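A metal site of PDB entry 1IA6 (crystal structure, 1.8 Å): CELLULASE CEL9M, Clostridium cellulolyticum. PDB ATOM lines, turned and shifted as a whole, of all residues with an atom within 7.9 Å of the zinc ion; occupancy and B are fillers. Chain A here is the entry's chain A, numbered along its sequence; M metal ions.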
ATOM      1  N   ASN A  20       5.615  13.734   4.238  1.00  0.00           N
ATOM      2  CA  ASN A  20       6.798  14.527   3.935  1.00  0.00           C
ATOM      3  C   ASN A  20       6.798  15.225   2.580  1.00  0.00           C
ATOM      4  O   ASN A  20       7.782  15.868   2.221  1.00  0.00           O
ATOM      5  CB  ASN A  20       8.048  13.651   4.075  1.00  0.00           C
ATOM      6  CG  ASN A  20       8.484  13.494   5.534  1.00  0.00           C
ATOM      7  OD1 ASN A  20       7.642  13.474   6.434  1.00  0.00           O
ATOM      8  ND2 ASN A  20       9.782  13.373   5.757  1.00  0.00           N
ATOM      9  N   LYS A  21       5.694  15.108   1.846  1.00  0.00           N
ATOM     10  CA  LYS A  21       5.620  15.765   0.535  1.00  0.00           C
ATOM     11  C   LYS A  21       5.803  17.270   0.682  1.00  0.00           C
ATOM     12  O   LYS A  21       5.280  17.883   1.610  1.00  0.00           O
ATOM     13  CB  LYS A  21       4.297  15.429  -0.164  1.00  0.00           C
ATOM     14  CG  LYS A  21       4.298  14.012  -0.723  1.00  0.00           C
ATOM     15  CD  LYS A  21       3.016  13.648  -1.433  1.00  0.00           C
ATOM     16  CE  LYS A  21       3.118  12.237  -2.004  1.00  0.00           C
ATOM     17  NZ  LYS A  21       1.844  11.757  -2.595  1.00  0.00           N
ATOM     18  N   CYS A  22       6.565  17.839  -0.238  1.00  0.00           N
ATOM     19  CA  CYS A  22       6.873  19.262  -0.220  1.00  0.00           C
ATOM     20  C   CYS A  22       6.412  19.903  -1.533  1.00  0.00           C
ATOM     21  O   CYS A  22       6.376  19.243  -2.571  1.00  0.00           O
ATOM     22  CB  CYS A  22       8.388  19.422  -0.060  1.00  0.00           C
ATOM     23  SG  CYS A  22       9.027  21.095   0.117  1.00  0.00           S
ATOM     24  N   GLY A  23       6.064  21.181  -1.477  1.00  0.00           N
ATOM     25  CA  GLY A  23       5.647  21.874  -2.687  1.00  0.00           C
ATOM     26  C   GLY A  23       4.206  22.312  -2.744  1.00  0.00           C
ATOM     27  O   GLY A  23       3.402  21.990  -1.866  1.00  0.00           O
ATOM     28  N   PRO A  24       3.839  23.061  -3.801  1.00  0.00           N
ATOM     29  CA  PRO A  24       2.480  23.566  -4.001  1.00  0.00           C
ATOM     30  C   PRO A  24       1.428  22.461  -4.092  1.00  0.00           C
ATOM     31  O   PRO A  24       0.272  22.664  -3.729  1.00  0.00           O
ATOM     32  CB  PRO A  24       2.587  24.348  -5.311  1.00  0.00           C
ATOM     33  CG  PRO A  24       4.011  24.814  -5.310  1.00  0.00           C
ATOM     34  CD  PRO A  24       4.746  23.587  -4.834  1.00  0.00           C
ATOM     35  N   ALA A  26       1.686  19.456  -2.534  1.00  0.00           N
ATOM     36  CA  ALA A  26       1.889  18.520  -1.435  1.00  0.00           C
ATOM     37  C   ALA A  26       0.579  17.928  -0.911  1.00  0.00           C
ATOM     38  O   ALA A  26       0.527  16.746  -0.559  1.00  0.00           O
ATOM     39  CB  ALA A  26       2.651  19.199  -0.301  1.00  0.00           C
ATOM     40  N   ARG A  35      -1.842  18.045   6.047  1.00  0.00           N
ATOM     41  CA  ARG A  35      -0.743  18.475   5.177  1.00  0.00           C
ATOM     42  C   ARG A  35      -1.276  19.334   4.044  1.00  0.00           C
ATOM     43  O   ARG A  35      -2.355  19.056   3.490  1.00  0.00           O
ATOM     44  CB  ARG A  35       0.003  17.274   4.575  1.00  0.00           C
ATOM     45  CG  ARG A  35       0.991  16.571   5.516  1.00  0.00           C
ATOM     46  CD  ARG A  35       1.954  17.553   6.173  1.00  0.00           C
ATOM     47  NE  ARG A  35       2.359  18.648   5.282  1.00  0.00           N
ATOM     48  CZ  ARG A  35       3.224  18.523   4.276  1.00  0.00           C
ATOM     49  NH1 ARG A  35       3.813  17.361   4.019  1.00  0.00           N
ATOM     50  NH2 ARG A  35       3.480  19.581   3.514  1.00  0.00           N
ATOM     51  N   GLY A  36      -0.537  20.386   3.705  1.00  0.00           N
ATOM     52  CA  GLY A  36      -0.941  21.276   2.637  1.00  0.00           C
ATOM     53  C   GLY A  36       0.270  21.811   1.882  1.00  0.00           C
ATOM     54  O   GLY A  36       1.386  21.351   2.097  1.00  0.00           O
ATOM     55  N   ALA A  37       0.047  22.799   1.024  1.00  0.00           N
ATOM     56  CA  ALA A  37       1.132  23.400   0.249  1.00  0.00           C
ATOM     57  C   ALA A  37       2.205  24.012   1.140  1.00  0.00           C
ATOM     58  O   ALA A  37       1.885  24.683   2.129  1.00  0.00           O
ATOM     59  CB  ALA A  37       0.577  24.460  -0.703  1.00  0.00           C
ATOM     60  N   CYS A  38       3.463  23.798   0.790  1.00  0.00           N
ATOM     61  CA  CYS A  38       4.580  24.344   1.561  1.00  0.00           C
ATOM     62  C   CYS A  38       5.763  24.680   0.648  1.00  0.00           C
ATOM     63  O   CYS A  38       5.861  24.159  -0.461  1.00  0.00           O
ATOM     64  CB  CYS A  38       5.020  23.346   2.634  1.00  0.00           C
ATOM     65  SG  CYS A  38       5.616  21.746   1.995  1.00  0.00           S
ATOM     66  N   HIS A  39       6.653  25.543   1.141  1.00  0.00           N
ATOM     67  CA  HIS A  39       7.860  25.942   0.413  1.00  0.00           C
ATOM     68  C   HIS A  39       7.599  26.045  -1.087  1.00  0.00           C
ATOM     69  O   HIS A  39       8.294  25.429  -1.902  1.00  0.00           O
ATOM     70  CB  HIS A  39       8.966  24.932   0.704  1.00  0.00           C
ATOM     71  CG  HIS A  39       9.131  24.636   2.168  1.00  0.00           C
ATOM     72  ND1 HIS A  39       8.673  23.474   2.741  1.00  0.00           N
ATOM     73  CD2 HIS A  39       9.646  25.379   3.175  1.00  0.00           C
ATOM     74  CE1 HIS A  39       8.913  23.507   4.045  1.00  0.00           C
ATOM     75  NE2 HIS A  39       9.499  24.652   4.332  1.00  0.00           N
ATOM     76  N   THR A  40       6.615  26.850  -1.431  1.00  0.00           N
ATOM     77  CA  THR A  40       6.197  27.049  -2.817  1.00  0.00           C
ATOM     78  C   THR A  40       7.113  27.910  -3.670  1.00  0.00           C
ATOM     79  O   THR A  40       6.854  28.072  -4.864  1.00  0.00           O
ATOM     80  CB  THR A  40       4.785  27.650  -2.853  1.00  0.00           C
ATOM     81  OG1 THR A  40       4.803  28.934  -2.214  1.00  0.00           O
ATOM     82  CG2 THR A  40       3.800  26.753  -2.123  1.00  0.00           C
ATOM     83  N   ASP A  42      10.620  27.440  -3.652  1.00  0.00           N
ATOM     84  CA  ASP A  42      11.923  26.784  -3.769  1.00  0.00           C
ATOM     85  C   ASP A  42      12.551  26.980  -5.149  1.00  0.00           C
ATOM     86  O   ASP A  42      11.896  26.780  -6.166  1.00  0.00           O
ATOM     87  CB  ASP A  42      11.792  25.293  -3.485  1.00  0.00           C
ATOM     88  CG  ASP A  42      11.656  24.986  -2.007  1.00  0.00           C
ATOM     89  OD1 ASP A  42      11.723  25.935  -1.185  1.00  0.00           O
ATOM     90  OD2 ASP A  42      11.469  23.798  -1.660  1.00  0.00           O
ATOM     91  N   GLY A  52       8.624  20.719  -4.974  1.00  0.00           N
ATOM     92  CA  GLY A  52       8.305  19.300  -5.045  1.00  0.00           C
ATOM     93  C   GLY A  52       9.280  18.488  -4.221  1.00  0.00           C
ATOM     94  O   GLY A  52      10.017  19.035  -3.397  1.00  0.00           O
ATOM     95  N   GLY A  53       9.301  17.184  -4.438  1.00  0.00           N
ATOM     96  CA  GLY A  53      10.201  16.346  -3.683  1.00  0.00           C
ATOM     97  C   GLY A  53       9.697  16.146  -2.267  1.00  0.00           C
ATOM     98  O   GLY A  53       8.536  16.447  -1.968  1.00  0.00           O
ATOM     99  N   TYR A  54      10.566  15.655  -1.383  1.00  0.00           N
ATOM    100  CA  TYR A  54      10.167  15.384  -0.013  1.00  0.00           C
ATOM    101  C   TYR A  54      11.080  15.965   1.055  1.00  0.00           C
ATOM    102  O   TYR A  54      12.289  16.073   0.867  1.00  0.00           O
ATOM    103  CB  TYR A  54      10.122  13.869   0.220  1.00  0.00           C
ATOM    104  CG  TYR A  54       9.124  13.094  -0.601  1.00  0.00           C
ATOM    105  CD1 TYR A  54       9.381  12.778  -1.938  1.00  0.00           C
ATOM    106  CD2 TYR A  54       7.942  12.621  -0.029  1.00  0.00           C
ATOM    107  CE1 TYR A  54       8.484  11.999  -2.674  1.00  0.00           C
ATOM    108  CE2 TYR A  54       7.053  11.841  -0.743  1.00  0.00           C
ATOM    109  CZ  TYR A  54       7.333  11.528  -2.071  1.00  0.00           C
ATOM    110  OH  TYR A  54       6.456  10.726  -2.763  1.00  0.00           O
ATOM    111  N   HIS A  55      10.482  16.309   2.191  1.00  0.00           N
ATOM    112  CA  HIS A  55      11.241  16.790   3.336  1.00  0.00           C
ATOM    113  C   HIS A  55      12.012  15.540   3.740  1.00  0.00           C
ATOM    114  O   HIS A  55      11.477  14.437   3.676  1.00  0.00           O
ATOM    115  CB  HIS A  55      10.300  17.198   4.464  1.00  0.00           C
ATOM    116  CG  HIS A  55       9.381  18.322   4.120  1.00  0.00           C
ATOM    117  ND1 HIS A  55       8.105  18.437   4.626  1.00  0.00           N
ATOM    118  CD2 HIS A  55       9.557  19.393   3.310  1.00  0.00           C
ATOM    119  CE1 HIS A  55       7.532  19.520   4.153  1.00  0.00           C
ATOM    120  NE2 HIS A  55       8.394  20.129   3.345  1.00  0.00           N
ATOM    121  N   ASP A  59      12.562  17.201   9.731  1.00  0.00           N
ATOM    122  CA  ASP A  59      12.854  18.561   9.324  1.00  0.00           C
ATOM    123  C   ASP A  59      12.302  18.797   7.917  1.00  0.00           C
ATOM    124  O   ASP A  59      11.578  17.956   7.379  1.00  0.00           O
ATOM    125  CB  ASP A  59      14.367  18.826   9.354  1.00  0.00           C
ATOM    126  CG  ASP A  59      15.160  17.800   8.561  1.00  0.00           C
ATOM    127  OD1 ASP A  59      14.543  16.925   7.933  1.00  0.00           O
ATOM    128  OD2 ASP A  59      16.405  17.889   8.576  1.00  0.00           O
ATOM    129  N   HIS A  60      12.668  19.922   7.312  1.00  0.00           N
ATOM    130  CA  HIS A  60      12.130  20.250   6.004  1.00  0.00           C
ATOM    131  C   HIS A  60      13.129  20.435   4.862  1.00  0.00           C
ATOM    132  O   HIS A  60      12.738  20.806   3.757  1.00  0.00           O
ATOM    133  CB  HIS A  60      11.256  21.501   6.132  1.00  0.00           C
ATOM    134  CG  HIS A  60      10.154  21.353   7.139  1.00  0.00           C
ATOM    135  ND1 HIS A  60       9.779  22.371   8.001  1.00  0.00           N
ATOM    136  CD2 HIS A  60       9.351  20.299   7.428  1.00  0.00           C
ATOM    137  CE1 HIS A  60       8.792  21.941   8.766  1.00  0.00           C
ATOM    138  NE2 HIS A  60       8.515  20.692   8.454  1.00  0.00           N
ATOM    139  N   VAL A  61      14.397  20.167   5.127  1.00  0.00           N
ATOM    140  CA  VAL A  61      15.417  20.301   4.106  1.00  0.00           C
ATOM    141  C   VAL A  61      15.336  19.128   3.133  1.00  0.00           C
ATOM    142  O   VAL A  61      14.981  18.010   3.520  1.00  0.00           O
ATOM    143  CB  VAL A  61      16.823  20.326   4.740  1.00  0.00           C
ATOM    144  CG1 VAL A  61      17.897  20.377   3.648  1.00  0.00           C
ATOM    145  CG2 VAL A  61      16.945  21.511   5.672  1.00  0.00           C
ATOM    146  N   LYS A  62      15.644  19.376   1.867  1.00  0.00           N
ATOM    147  CA  LYS A  62      15.643  18.321   0.864  1.00  0.00           C
ATOM    148  C   LYS A  62      17.118  18.023   0.576  1.00  0.00           C
ATOM    149  O   LYS A  62      17.777  18.779  -0.131  1.00  0.00           O
ATOM    150  CB  LYS A  62      14.888  18.777  -0.393  1.00  0.00           C
ATOM    151  CG  LYS A  62      13.439  19.173  -0.064  1.00  0.00           C
ATOM    152  CD  LYS A  62      12.581  19.451  -1.288  1.00  0.00           C
ATOM    153  CE  LYS A  62      12.926  20.758  -1.962  1.00  0.00           C
ATOM    154  NZ  LYS A  62      11.866  21.154  -2.934  1.00  0.00           N
ATOM    155  N   TYR A 100       6.314  11.439  -7.621  1.00  0.00           N
ATOM    156  CA  TYR A 100       6.520  12.705  -6.914  1.00  0.00           C
ATOM    157  C   TYR A 100       8.025  12.924  -6.774  1.00  0.00           C
ATOM    158  O   TYR A 100       8.500  14.063  -6.804  1.00  0.00           O
ATOM    159  CB  TYR A 100       5.863  12.678  -5.543  1.00  0.00           C
ATOM    160  CG  TYR A 100       5.475  14.063  -5.048  1.00  0.00           C
ATOM    161  CD1 TYR A 100       4.338  14.705  -5.550  1.00  0.00           C
ATOM    162  CD2 TYR A 100       6.258  14.745  -4.123  1.00  0.00           C
ATOM    163  CE1 TYR A 100       3.996  15.991  -5.124  1.00  0.00           C
ATOM    164  CE2 TYR A 100       5.927  16.027  -3.688  1.00  0.00           C
ATOM    165  CZ  TYR A 100       4.793  16.648  -4.192  1.00  0.00           C
ATOM    166  OH  TYR A 100       4.455  17.928  -3.794  1.00  0.00           O
ATOM    167  N   PRO A 132       5.286  22.884   8.222  1.00  0.00           N
ATOM    168  CA  PRO A 132       6.034  23.315   7.032  1.00  0.00           C
ATOM    169  C   PRO A 132       5.258  24.337   6.224  1.00  0.00           C
ATOM    170  O   PRO A 132       5.839  25.176   5.548  1.00  0.00           O
ATOM    171  CB  PRO A 132       6.264  22.008   6.272  1.00  0.00           C
ATOM    172  CG  PRO A 132       5.100  21.152   6.692  1.00  0.00           C
ATOM    173  CD  PRO A 132       5.009  21.447   8.175  1.00  0.00           C
ATOM    174  N   GLU A 133       3.927  24.273   6.303  1.00  0.00           N
ATOM    175  CA  GLU A 133       3.074  25.200   5.564  1.00  0.00           C
ATOM    176  C   GLU A 133       3.215  26.639   6.039  1.00  0.00           C
ATOM    177  O   GLU A 133       2.921  27.580   5.285  1.00  0.00           O
ATOM    178  CB  GLU A 133       1.599  24.784   5.685  1.00  0.00           C
ATOM    179  CG  GLU A 133       1.245  23.436   5.067  1.00  0.00           C
ATOM    180  CD  GLU A 133       1.599  22.258   5.956  1.00  0.00           C
ATOM    181  OE1 GLU A 133       2.053  22.485   7.098  1.00  0.00           O
ATOM    182  OE2 GLU A 133       1.423  21.102   5.513  1.00  0.00           O
ATOM    183  N   GLN A 135       6.189  27.867   7.380  1.00  0.00           N
ATOM    184  CA  GLN A 135       7.603  28.235   7.385  1.00  0.00           C
ATOM    185  C   GLN A 135       7.830  29.108   6.164  1.00  0.00           C
ATOM    186  O   GLN A 135       7.989  28.607   5.050  1.00  0.00           O
ATOM    187  CB  GLN A 135       8.477  26.984   7.344  1.00  0.00           C
ATOM    188  CG  GLN A 135       9.963  27.267   7.367  1.00  0.00           C
ATOM    189  CD  GLN A 135      10.775  25.998   7.519  1.00  0.00           C
ATOM    190  OE1 GLN A 135      10.426  24.962   6.967  1.00  0.00           O
ATOM    191  NE2 GLN A 135      11.875  26.081   8.266  1.00  0.00           N
ATOM    192  N   ARG A 139      14.476  29.810   1.158  1.00  0.00           N
ATOM    193  CA  ARG A 139      15.353  28.658   1.307  1.00  0.00           C
ATOM    194  C   ARG A 139      16.377  28.725   0.199  1.00  0.00           C
ATOM    195  O   ARG A 139      16.033  28.954  -0.959  1.00  0.00           O
ATOM    196  CB  ARG A 139      14.565  27.353   1.191  1.00  0.00           C
ATOM    197  CG  ARG A 139      14.158  26.747   2.513  1.00  0.00           C
ATOM    198  CD  ARG A 139      12.696  26.362   2.499  1.00  0.00           C
ATOM    199  NE  ARG A 139      12.385  25.283   1.568  1.00  0.00           N
ATOM    200  CZ  ARG A 139      12.432  23.982   1.883  1.00  0.00           C
ATOM    201  NH1 ARG A 139      12.808  23.610   3.103  1.00  0.00           N
ATOM    202  NH2 ARG A 139      12.079  23.065   0.987  1.00  0.00           N
HETATM  203 ZN    ZN M   1       7.921  21.678   2.026  1.00  0.00          ZN
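A ring nitrogen (NE2) of His 39 is in hydrogen-bond range of the side-chain amide oxygen of Gln 135. O of Asn 20 sits at hydrogen-bond distance from N of His 55 (2.7 Å). The side-chain sulfur (SG) of Cys 22 sits close to the guanidinium group (NH2) of Arg 139, at 3.7 Å. O of Gly 53 sits at hydrogen-bond distance from N of Cys 22, at 3.0 Å. The backbone carbonyl oxygen (O) of Cys 22 sits at hydrogen-bond distance from the side-chain hydroxyl (OH) of Tyr 100 (2.6 Å). The backbone carbonyl oxygen (O) of Cys 38 is in hydrogen-bond range of the backbone NH (N) of Gly 23. NH2 of Arg 35 lies close to SG of Cys 38 (3.4 Å).
Residues that only touch the zinc ion: Gly 23 (3.996 Å). Within 4 Å of the zinc ion: Cys 22, Gly 23, Cys 38, His 39 and His 55.
The zinc ion is bound by a ring nitrogen (ND1) of His 39 (2.1 Å), a ring nitrogen (NE2) of His 55 (2.1 Å), the side-chain sulfur of Cys 22 (2.3 Å) and the side-chain sulfur of Cys 38 (2.3 Å).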
